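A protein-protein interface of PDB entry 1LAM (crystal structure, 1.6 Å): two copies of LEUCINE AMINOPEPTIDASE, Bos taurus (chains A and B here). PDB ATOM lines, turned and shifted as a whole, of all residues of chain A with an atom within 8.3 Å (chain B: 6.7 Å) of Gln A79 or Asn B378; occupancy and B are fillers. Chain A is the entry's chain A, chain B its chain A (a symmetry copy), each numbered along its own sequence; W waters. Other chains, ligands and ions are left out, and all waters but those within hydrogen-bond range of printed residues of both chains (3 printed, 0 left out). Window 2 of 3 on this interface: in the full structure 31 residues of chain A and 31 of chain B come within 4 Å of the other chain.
Water W1 lies within hydrogen-bond range of the side-chain carboxylate of Glu A80 (2.8 Å), the side-chain amino group of Lys B437 (3.2 Å) and the backbone carbonyl oxygen of Leu B402 (3.4 Å). Water W3 lies within hydrogen-bond range of the guanidinium group of Arg B399 (2.8 Å), the side-chain amide oxygen of Gln A79 (3.0 Å) and the backbone carbonyl oxygen of Asn B378 (3.5 Å). Water W2 bridges O of Arg B399 (3.0 Å) and NE1 of Trp A398 (3.1 Å).
No position is printed for both chains. Of the 7 pairs that touch across the chains among the printed residues, none has its exchanged pair printed and touching as well.
Of chain B, only Asn B378 (2.9 Å), Leu B402 (3.9 Å) and Phe B403 (3.8 Å) come within 4 Å of Gln A79. Asn B378 touches one residue of chain A. Of the printed residues of chain B, Glu A80 touches Phe B403 (3.4 Å). Of the printed residues of chain A, Arg B399 touches Trp A398 (2.8 Å). Of the printed residues of chain B, Trp A398 touches Arg B399 and Phe B403. Of the printed residues of chain A, Leu B402 touches Gln A79. Printed residues of chain A within 4 Å of Phe B403: Gln A79 (3.8 Å), Glu A80 (3.4 Å), Arg A396 (3.3 Å) and Trp A398 (3.9 Å). The nearest residue of chain B that does not touch Gln A79 is Thr B377 (4.5 Å).
Printed residues of chain B that touch a printed residue of chain A: Asn B378, Arg B399, Leu B402 and Phe B403. Printed residues of chain A that touch a printed residue of chain B: Gln A79, Glu A80, Arg A396 and Trp A398. Hydrophobic or aromatic side chains of chain A that line the printed part of chain B: Trp A398. Among the printed residues, no Asp or Glu carboxylate lies within 4 Å of a Lys or Arg side-chain nitrogen of the other chain.
The backbone carbonyl oxygen of Asn B378 is in hydrogen-bond range of the side-chain amide nitrogen of Gln A79 (2.9 Å). NE1 of Trp A398 is in hydrogen-bond range of O of Arg B399, 2.8 Å away.
Among the printed residues, pairs that only touch across the chains: Arg A396 with Phe B403, Glu A80 with Phe B403, Gln A79 with Phe B403, Gln A79 with Leu B402 and Trp A398 with Phe B403.
N of Glu A80 is in hydrogen-bond range of OD1 of Asp A77, at 3.4 Å. The side-chain carboxylate (OE1) of Glu A80 lies within salt-bridge range of the guanidinium group (NH1) of Arg A396, at 2.8 Å. The backbone carbonyl oxygen of Thr B377 sits at hydrogen-bond distance from the guanidinium group of Arg B399 (3.0 Å). The side-chain amide nitrogen (ND2) of Asn B378 sits at hydrogen-bond distance from the backbone carbonyl oxygen (O) of His B442 (2.9 Å). The side-chain amide oxygen (OD1) of Asn B378 lies within hydrogen-bond range of the backbone NH (N) of Trp B445, at 3.0 Å. OG of Ser B380 is in hydrogen-bond range of NH1 of Arg B399 (3.0 Å).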
ATOM      1  N   ILE A  76     -27.330  -0.030  28.333  1.00  0.00           N
ATOM      2  CA  ILE A  76     -26.963   1.368  28.355  1.00  0.00           C
ATOM      3  C   ILE A  76     -25.816   1.620  27.390  1.00  0.00           C
ATOM      4  O   ILE A  76     -24.802   0.909  27.409  1.00  0.00           O
ATOM      5  CB  ILE A  76     -26.592   1.842  29.765  1.00  0.00           C
ATOM      6  CG1 ILE A  76     -27.846   1.855  30.654  1.00  0.00           C
ATOM      7  CG2 ILE A  76     -25.975   3.237  29.696  1.00  0.00           C
ATOM      8  CD1 ILE A  76     -27.597   2.252  32.090  1.00  0.00           C
ATOM      9  N   ASP A  77     -26.021   2.579  26.496  1.00  0.00           N
ATOM     10  CA  ASP A  77     -25.019   2.949  25.522  1.00  0.00           C
ATOM     11  C   ASP A  77     -24.209   4.076  26.165  1.00  0.00           C
ATOM     12  O   ASP A  77     -24.715   5.180  26.389  1.00  0.00           O
ATOM     13  CB  ASP A  77     -25.689   3.417  24.222  1.00  0.00           C
ATOM     14  CG  ASP A  77     -24.689   3.695  23.106  1.00  0.00           C
ATOM     15  OD1 ASP A  77     -23.526   4.061  23.391  1.00  0.00           O
ATOM     16  OD2 ASP A  77     -25.075   3.570  21.925  1.00  0.00           O
ATOM     17  N   GLU A  78     -22.956   3.763  26.467  1.00  0.00           N
ATOM     18  CA  GLU A  78     -22.012   4.673  27.096  1.00  0.00           C
ATOM     19  C   GLU A  78     -21.841   5.987  26.320  1.00  0.00           C
ATOM     20  O   GLU A  78     -21.643   7.050  26.907  1.00  0.00           O
ATOM     21  CB  GLU A  78     -20.641   3.991  27.207  1.00  0.00           C
ATOM     22  CG  GLU A  78     -20.643   2.549  27.785  1.00  0.00           C
ATOM     23  CD  GLU A  78     -20.981   1.398  26.767  1.00  0.00           C
ATOM     24  OE1 GLU A  78     -21.245   1.644  25.552  1.00  0.00           O
ATOM     25  OE2 GLU A  78     -20.967   0.219  27.224  1.00  0.00           O
ATOM     26  N   GLN A  79     -21.848   5.901  24.994  1.00  0.00           N
ATOM     27  CA  GLN A  79     -21.679   7.081  24.151  1.00  0.00           C
ATOM     28  C   GLN A  79     -22.939   7.932  23.981  1.00  0.00           C
ATOM     29  O   GLN A  79     -22.845   9.147  23.835  1.00  0.00           O
ATOM     30  CB  GLN A  79     -21.177   6.659  22.764  1.00  0.00           C
ATOM     31  CG  GLN A  79     -19.863   5.894  22.778  1.00  0.00           C
ATOM     32  CD  GLN A  79     -18.710   6.689  23.376  1.00  0.00           C
ATOM     33  OE1 GLN A  79     -18.693   7.922  23.327  1.00  0.00           O
ATOM     34  NE2 GLN A  79     -17.742   5.992  23.932  1.00  0.00           N
ATOM     35  N   GLU A  80     -24.109   7.304  24.032  1.00  0.00           N
ATOM     36  CA  GLU A  80     -25.358   8.023  23.819  1.00  0.00           C
ATOM     37  C   GLU A  80     -26.084   8.446  25.097  1.00  0.00           C
ATOM     38  O   GLU A  80     -27.052   9.215  25.046  1.00  0.00           O
ATOM     39  CB  GLU A  80     -26.293   7.208  22.917  1.00  0.00           C
ATOM     40  CG  GLU A  80     -25.734   6.888  21.524  1.00  0.00           C
ATOM     41  CD  GLU A  80     -25.693   8.097  20.595  1.00  0.00           C
ATOM     42  OE1 GLU A  80     -26.331   9.128  20.898  1.00  0.00           O
ATOM     43  OE2 GLU A  80     -25.017   8.018  19.552  1.00  0.00           O
ATOM     44  N   ASN A  81     -25.616   7.953  26.239  1.00  0.00           N
ATOM     45  CA  ASN A  81     -26.220   8.290  27.525  1.00  0.00           C
ATOM     46  C   ASN A  81     -27.706   7.921  27.629  1.00  0.00           C
ATOM     47  O   ASN A  81     -28.522   8.711  28.129  1.00  0.00           O
ATOM     48  CB  ASN A  81     -26.038   9.776  27.869  1.00  0.00           C
ATOM     49  CG  ASN A  81     -24.576  10.204  27.986  1.00  0.00           C
ATOM     50  OD1 ASN A  81     -24.248  11.373  27.748  1.00  0.00           O
ATOM     51  ND2 ASN A  81     -23.717   9.298  28.376  1.00  0.00           N
ATOM     52  N   TRP A  82     -28.070   6.749  27.114  1.00  0.00           N
ATOM     53  CA  TRP A  82     -29.442   6.266  27.235  1.00  0.00           C
ATOM     54  C   TRP A  82     -29.455   4.747  27.168  1.00  0.00           C
ATOM     55  O   TRP A  82     -28.433   4.123  26.853  1.00  0.00           O
ATOM     56  CB  TRP A  82     -30.398   6.863  26.183  1.00  0.00           C
ATOM     57  CG  TRP A  82     -30.125   6.548  24.722  1.00  0.00           C
ATOM     58  CD1 TRP A  82     -29.328   5.562  24.209  1.00  0.00           C
ATOM     59  CD2 TRP A  82     -30.653   7.261  23.596  1.00  0.00           C
ATOM     60  NE1 TRP A  82     -29.313   5.619  22.834  1.00  0.00           N
ATOM     61  CE2 TRP A  82     -30.119   6.663  22.429  1.00  0.00           C
ATOM     62  CE3 TRP A  82     -31.518   8.361  23.454  1.00  0.00           C
ATOM     63  CZ2 TRP A  82     -30.426   7.115  21.140  1.00  0.00           C
ATOM     64  CZ3 TRP A  82     -31.824   8.819  22.175  1.00  0.00           C
ATOM     65  CH2 TRP A  82     -31.275   8.197  21.035  1.00  0.00           C
ATOM     66  N   ARG A 396     -33.189  12.724  26.838  1.00  0.00           N
ATOM     67  CA  ARG A 396     -31.922  13.229  27.349  1.00  0.00           C
ATOM     68  C   ARG A 396     -31.774  14.658  27.845  1.00  0.00           C
ATOM     69  O   ARG A 396     -32.462  15.571  27.387  1.00  0.00           O
ATOM     70  CB  ARG A 396     -30.818  12.896  26.341  1.00  0.00           C
ATOM     71  CG  ARG A 396     -30.767  11.417  25.964  1.00  0.00           C
ATOM     72  CD  ARG A 396     -29.637  11.106  24.984  1.00  0.00           C
ATOM     73  NE  ARG A 396     -29.940  11.503  23.600  1.00  0.00           N
ATOM     74  CZ  ARG A 396     -29.251  11.091  22.538  1.00  0.00           C
ATOM     75  NH1 ARG A 396     -28.198  10.294  22.699  1.00  0.00           N
ATOM     76  NH2 ARG A 396     -29.602  11.489  21.319  1.00  0.00           N
ATOM     77  N   TRP A 398     -28.535  17.532  29.231  1.00  0.00           N
ATOM     78  CA  TRP A 398     -27.105  17.834  29.057  1.00  0.00           C
ATOM     79  C   TRP A 398     -26.816  19.058  29.916  1.00  0.00           C
ATOM     80  O   TRP A 398     -27.529  20.050  29.807  1.00  0.00           O
ATOM     81  CB  TRP A 398     -26.813  18.143  27.573  1.00  0.00           C
ATOM     82  CG  TRP A 398     -25.363  18.196  27.280  1.00  0.00           C
ATOM     83  CD1 TRP A 398     -24.557  19.301  27.321  1.00  0.00           C
ATOM     84  CD2 TRP A 398     -24.502  17.088  27.034  1.00  0.00           C
ATOM     85  NE1 TRP A 398     -23.244  18.944  27.138  1.00  0.00           N
ATOM     86  CE2 TRP A 398     -23.181  17.582  26.956  1.00  0.00           C
ATOM     87  CE3 TRP A 398     -24.718  15.708  26.871  1.00  0.00           C
ATOM     88  CZ2 TRP A 398     -22.073  16.755  26.730  1.00  0.00           C
ATOM     89  CZ3 TRP A 398     -23.615  14.880  26.644  1.00  0.00           C
ATOM     90  CH2 TRP A 398     -22.311  15.411  26.579  1.00  0.00           C
ATOM     91  N   PHE B 376     -15.843  17.980  22.508  1.00  0.00           N
ATOM     92  CA  PHE B 376     -16.611  16.835  22.013  1.00  0.00           C
ATOM     93  C   PHE B 376     -15.648  15.649  22.057  1.00  0.00           C
ATOM     94  O   PHE B 376     -14.599  15.685  21.414  1.00  0.00           O
ATOM     95  CB  PHE B 376     -17.056  17.073  20.565  1.00  0.00           C
ATOM     96  CG  PHE B 376     -18.064  18.184  20.403  1.00  0.00           C
ATOM     97  CD1 PHE B 376     -17.654  19.504  20.210  1.00  0.00           C
ATOM     98  CD2 PHE B 376     -19.431  17.904  20.409  1.00  0.00           C
ATOM     99  CE1 PHE B 376     -18.583  20.537  20.016  1.00  0.00           C
ATOM    100  CE2 PHE B 376     -20.377  18.933  20.212  1.00  0.00           C
ATOM    101  CZ  PHE B 376     -19.943  20.255  20.016  1.00  0.00           C
ATOM    102  N   THR B 377     -15.982  14.596  22.794  1.00  0.00           N
ATOM    103  CA  THR B 377     -15.073  13.454  22.866  1.00  0.00           C
ATOM    104  C   THR B 377     -15.771  12.107  23.045  1.00  0.00           C
ATOM    105  O   THR B 377     -16.806  12.015  23.705  1.00  0.00           O
ATOM    106  CB  THR B 377     -13.980  13.643  23.980  1.00  0.00           C
ATOM    107  OG1 THR B 377     -13.096  12.508  24.002  1.00  0.00           O
ATOM    108  CG2 THR B 377     -14.608  13.842  25.359  1.00  0.00           C
ATOM    109  N   ASN B 378     -15.184  11.070  22.446  1.00  0.00           N
ATOM    110  CA  ASN B 378     -15.739   9.721  22.550  1.00  0.00           C
ATOM    111  C   ASN B 378     -15.128   8.966  23.730  1.00  0.00           C
ATOM    112  O   ASN B 378     -15.402   7.784  23.927  1.00  0.00           O
ATOM    113  CB  ASN B 378     -15.520   8.928  21.253  1.00  0.00           C
ATOM    114  CG  ASN B 378     -14.052   8.787  20.856  1.00  0.00           C
ATOM    115  OD1 ASN B 378     -13.151   9.297  21.516  1.00  0.00           O
ATOM    116  ND2 ASN B 378     -13.817   8.086  19.766  1.00  0.00           N
ATOM    117  N   SER B 379     -14.372   9.687  24.553  1.00  0.00           N
ATOM    118  CA  SER B 379     -13.697   9.104  25.694  1.00  0.00           C
ATOM    119  C   SER B 379     -13.861   9.920  26.973  1.00  0.00           C
ATOM    120  O   SER B 379     -13.326  11.035  27.100  1.00  0.00           O
ATOM    121  CB  SER B 379     -12.207   8.943  25.351  1.00  0.00           C
ATOM    122  OG  SER B 379     -11.425   8.623  26.493  1.00  0.00           O
ATOM    123  N   SER B 380     -14.586   9.359  27.936  1.00  0.00           N
ATOM    124  CA  SER B 380     -14.784  10.034  29.216  1.00  0.00           C
ATOM    125  C   SER B 380     -13.465  10.168  29.986  1.00  0.00           C
ATOM    126  O   SER B 380     -13.291  11.117  30.747  1.00  0.00           O
ATOM    127  CB  SER B 380     -15.850   9.326  30.040  1.00  0.00           C
ATOM    128  OG  SER B 380     -17.112   9.533  29.423  1.00  0.00           O
ATOM    129  N   TRP B 381     -12.542   9.227  29.769  1.00  0.00           N
ATOM    130  CA  TRP B 381     -11.221   9.285  30.393  1.00  0.00           C
ATOM    131  C   TRP B 381     -10.510  10.562  29.893  1.00  0.00           C
ATOM    132  O   TRP B 381      -9.921  11.319  30.682  1.00  0.00           O
ATOM    133  CB  TRP B 381     -10.387   8.047  30.016  1.00  0.00           C
ATOM    134  CG  TRP B 381      -8.925   8.173  30.372  1.00  0.00           C
ATOM    135  CD1 TRP B 381      -8.337   7.851  31.563  1.00  0.00           C
ATOM    136  CD2 TRP B 381      -7.886   8.719  29.550  1.00  0.00           C
ATOM    137  NE1 TRP B 381      -7.003   8.184  31.539  1.00  0.00           N
ATOM    138  CE2 TRP B 381      -6.703   8.731  30.316  1.00  0.00           C
ATOM    139  CE3 TRP B 381      -7.848   9.236  28.249  1.00  0.00           C
ATOM    140  CZ2 TRP B 381      -5.488   9.204  29.821  1.00  0.00           C
ATOM    141  CZ3 TRP B 381      -6.642   9.711  27.756  1.00  0.00           C
ATOM    142  CH2 TRP B 381      -5.480   9.705  28.544  1.00  0.00           C
ATOM    143  N   LEU B 382     -10.572  10.784  28.581  1.00  0.00           N
ATOM    144  CA  LEU B 382      -9.949  11.946  27.956  1.00  0.00           C
ATOM    145  C   LEU B 382     -10.655  13.233  28.398  1.00  0.00           C
ATOM    146  O   LEU B 382      -9.984  14.227  28.705  1.00  0.00           O
ATOM    147  CB  LEU B 382      -9.957  11.794  26.441  1.00  0.00           C
ATOM    148  CG  LEU B 382      -9.230  12.869  25.639  1.00  0.00           C
ATOM    149  CD1 LEU B 382      -7.844  13.156  26.234  1.00  0.00           C
ATOM    150  CD2 LEU B 382      -9.139  12.417  24.178  1.00  0.00           C
ATOM    151  N   ARG B 399     -18.041  20.043  28.402  1.00  0.00           N
ATOM    152  CA  ARG B 399     -18.345  18.982  27.445  1.00  0.00           C
ATOM    153  C   ARG B 399     -19.599  19.232  26.626  1.00  0.00           C
ATOM    154  O   ARG B 399     -20.568  19.769  27.125  1.00  0.00           O
ATOM    155  CB  ARG B 399     -18.440  17.630  28.164  1.00  0.00           C
ATOM    156  CG  ARG B 399     -18.202  16.428  27.252  1.00  0.00           C
ATOM    157  CD  ARG B 399     -18.329  15.090  27.994  1.00  0.00           C
ATOM    158  NE  ARG B 399     -17.966  13.976  27.123  1.00  0.00           N
ATOM    159  CZ  ARG B 399     -17.815  12.710  27.514  1.00  0.00           C
ATOM    160  NH1 ARG B 399     -17.971  12.368  28.794  1.00  0.00           N
ATOM    161  NH2 ARG B 399     -17.474  11.790  26.622  1.00  0.00           N
ATOM    162  N   LEU B 402     -21.670  14.185  21.591  1.00  0.00           N
ATOM    163  CA  LEU B 402     -21.328  13.458  20.359  1.00  0.00           C
ATOM    164  C   LEU B 402     -22.401  12.368  20.216  1.00  0.00           C
ATOM    165  O   LEU B 402     -22.198  11.231  20.642  1.00  0.00           O
ATOM    166  CB  LEU B 402     -19.948  12.792  20.441  1.00  0.00           C
ATOM    167  CG  LEU B 402     -18.718  13.523  19.904  1.00  0.00           C
ATOM    168  CD1 LEU B 402     -17.549  12.575  19.979  1.00  0.00           C
ATOM    169  CD2 LEU B 402     -18.917  14.000  18.460  1.00  0.00           C
ATOM    170  N   PHE B 403     -23.547  12.736  19.644  1.00  0.00           N
ATOM    171  CA  PHE B 403     -24.683  11.815  19.491  1.00  0.00           C
ATOM    172  C   PHE B 403     -24.977  11.499  18.027  1.00  0.00           C
ATOM    173  O   PHE B 403     -24.853  12.382  17.166  1.00  0.00           O
ATOM    174  CB  PHE B 403     -25.961  12.450  20.065  1.00  0.00           C
ATOM    175  CG  PHE B 403     -25.972  12.645  21.568  1.00  0.00           C
ATOM    176  CD1 PHE B 403     -25.060  11.997  22.406  1.00  0.00           C
ATOM    177  CD2 PHE B 403     -26.947  13.469  22.148  1.00  0.00           C
ATOM    178  CE1 PHE B 403     -25.143  12.136  23.807  1.00  0.00           C
ATOM    179  CE2 PHE B 403     -27.044  13.616  23.541  1.00  0.00           C
ATOM    180  CZ  PHE B 403     -26.131  12.957  24.371  1.00  0.00           C
ATOM    181  N   LYS B 437     -16.349  13.489  13.222  1.00  0.00           N
ATOM    182  CA  LYS B 437     -16.333  12.106  13.697  1.00  0.00           C
ATOM    183  C   LYS B 437     -16.414  11.080  12.571  1.00  0.00           C
ATOM    184  O   LYS B 437     -15.956   9.944  12.724  1.00  0.00           O
ATOM    185  CB  LYS B 437     -17.439  11.866  14.729  1.00  0.00           C
ATOM    186  CG  LYS B 437     -17.289  10.549  15.448  1.00  0.00           C
ATOM    187  CD  LYS B 437     -18.263  10.383  16.609  1.00  0.00           C
ATOM    188  CE  LYS B 437     -19.726  10.467  16.177  1.00  0.00           C
ATOM    189  NZ  LYS B 437     -20.647  10.003  17.264  1.00  0.00           N
ATOM    190  N   VAL B 440     -12.992   9.852  11.890  1.00  0.00           N
ATOM    191  CA  VAL B 440     -12.225   9.355  13.028  1.00  0.00           C
ATOM    192  C   VAL B 440     -12.670   7.955  13.445  1.00  0.00           C
ATOM    193  O   VAL B 440     -13.866   7.695  13.563  1.00  0.00           O
ATOM    194  CB  VAL B 440     -12.397  10.297  14.266  1.00  0.00           C
ATOM    195  CG1 VAL B 440     -11.706   9.708  15.498  1.00  0.00           C
ATOM    196  CG2 VAL B 440     -11.834  11.685  13.966  1.00  0.00           C
ATOM    197  N   THR B 441     -11.713   7.047  13.610  1.00  0.00           N
ATOM    198  CA  THR B 441     -12.028   5.697  14.080  1.00  0.00           C
ATOM    199  C   THR B 441     -11.299   5.418  15.400  1.00  0.00           C
ATOM    200  O   THR B 441     -11.540   4.408  16.060  1.00  0.00           O
ATOM    201  CB  THR B 441     -11.627   4.625  13.063  1.00  0.00           C
ATOM    202  OG1 THR B 441     -10.237   4.772  12.751  1.00  0.00           O
ATOM    203  CG2 THR B 441     -12.439   4.770  11.794  1.00  0.00           C
ATOM    204  N   HIS B 442     -10.495   6.379  15.834  1.00  0.00           N
ATOM    205  CA  HIS B 442      -9.702   6.244  17.046  1.00  0.00           C
ATOM    206  C   HIS B 442     -10.586   6.254  18.285  1.00  0.00           C
ATOM    207  O   HIS B 442     -11.531   7.024  18.360  1.00  0.00           O
ATOM    208  CB  HIS B 442      -8.704   7.398  17.107  1.00  0.00           C
ATOM    209  CG  HIS B 442      -7.570   7.169  18.052  1.00  0.00           C
ATOM    210  ND1 HIS B 442      -7.665   7.428  19.403  1.00  0.00           N
ATOM    211  CD2 HIS B 442      -6.332   6.674  17.842  1.00  0.00           C
ATOM    212  CE1 HIS B 442      -6.526   7.088  19.989  1.00  0.00           C
ATOM    213  NE2 HIS B 442      -5.700   6.636  19.060  1.00  0.00           N
ATOM    214  N   PRO B 443     -10.251   5.437  19.300  1.00  0.00           N
ATOM    215  CA  PRO B 443     -11.031   5.359  20.549  1.00  0.00           C
ATOM    216  C   PRO B 443     -10.811   6.486  21.573  1.00  0.00           C
ATOM    217  O   PRO B 443     -11.530   6.577  22.571  1.00  0.00           O
ATOM    218  CB  PRO B 443     -10.614   4.000  21.130  1.00  0.00           C
ATOM    219  CG  PRO B 443      -9.180   3.883  20.688  1.00  0.00           C
ATOM    220  CD  PRO B 443      -9.260   4.344  19.243  1.00  0.00           C
ATOM    221  N   LYS B 444      -9.778   7.293  21.370  1.00  0.00           N
ATOM    222  CA  LYS B 444      -9.513   8.392  22.291  1.00  0.00           C
ATOM    223  C   LYS B 444      -9.275   9.678  21.517  1.00  0.00           C
ATOM    224  O   LYS B 444      -8.128  10.115  21.338  1.00  0.00           O
ATOM    225  CB  LYS B 444      -8.331   8.064  23.201  1.00  0.00           C
ATOM    226  CG  LYS B 444      -8.640   6.994  24.249  1.00  0.00           C
ATOM    227  CD  LYS B 444      -7.389   6.627  25.052  1.00  0.00           C
ATOM    228  CE  LYS B 444      -7.720   5.760  26.252  1.00  0.00           C
ATOM    229  NZ  LYS B 444      -8.472   4.531  25.844  1.00  0.00           N
ATOM    230  N   TRP B 445     -10.375  10.254  21.032  1.00  0.00           N
ATOM    231  CA  TRP B 445     -10.347  11.485  20.249  1.00  0.00           C
ATOM    232  C   TRP B 445     -11.152  12.592  20.923  1.00  0.00           C
ATOM    233  O   TRP B 445     -12.209  12.333  21.511  1.00  0.00           O
ATOM    234  CB  TRP B 445     -10.925  11.215  18.850  1.00  0.00           C
ATOM    235  CG  TRP B 445     -11.290  12.466  18.047  1.00  0.00           C
ATOM    236  CD1 TRP B 445     -10.428  13.399  17.543  1.00  0.00           C
ATOM    237  CD2 TRP B 445     -12.613  12.903  17.670  1.00  0.00           C
ATOM    238  NE1 TRP B 445     -11.128  14.384  16.878  1.00  0.00           N
ATOM    239  CE2 TRP B 445     -12.469  14.103  16.937  1.00  0.00           C
ATOM    240  CE3 TRP B 445     -13.907  12.393  17.881  1.00  0.00           C
ATOM    241  CZ2 TRP B 445     -13.564  14.805  16.415  1.00  0.00           C
ATOM    242  CZ3 TRP B 445     -14.999  13.097  17.357  1.00  0.00           C
ATOM    243  CH2 TRP B 445     -14.814  14.289  16.633  1.00  0.00           C
ATOM    244  N   ALA B 446     -10.634  13.815  20.865  1.00  0.00           N
ATOM    245  CA  ALA B 446     -11.315  14.978  21.419  1.00  0.00           C
ATOM    246  C   ALA B 446     -11.211  16.119  20.421  1.00  0.00           C
ATOM    247  O   ALA B 446     -10.146  16.359  19.845  1.00  0.00           O
ATOM    248  CB  ALA B 446     -10.697  15.395  22.732  1.00  0.00           C
HETATM  249  O   HOH W   1     -22.196   8.112  19.366  1.00  0.00           O
HETATM  250  O   HOH W   2     -21.762  19.228  29.876  1.00  0.00           O
HETATM  251  O   HOH W   3     -17.876   9.034  26.040  1.00  0.00           O
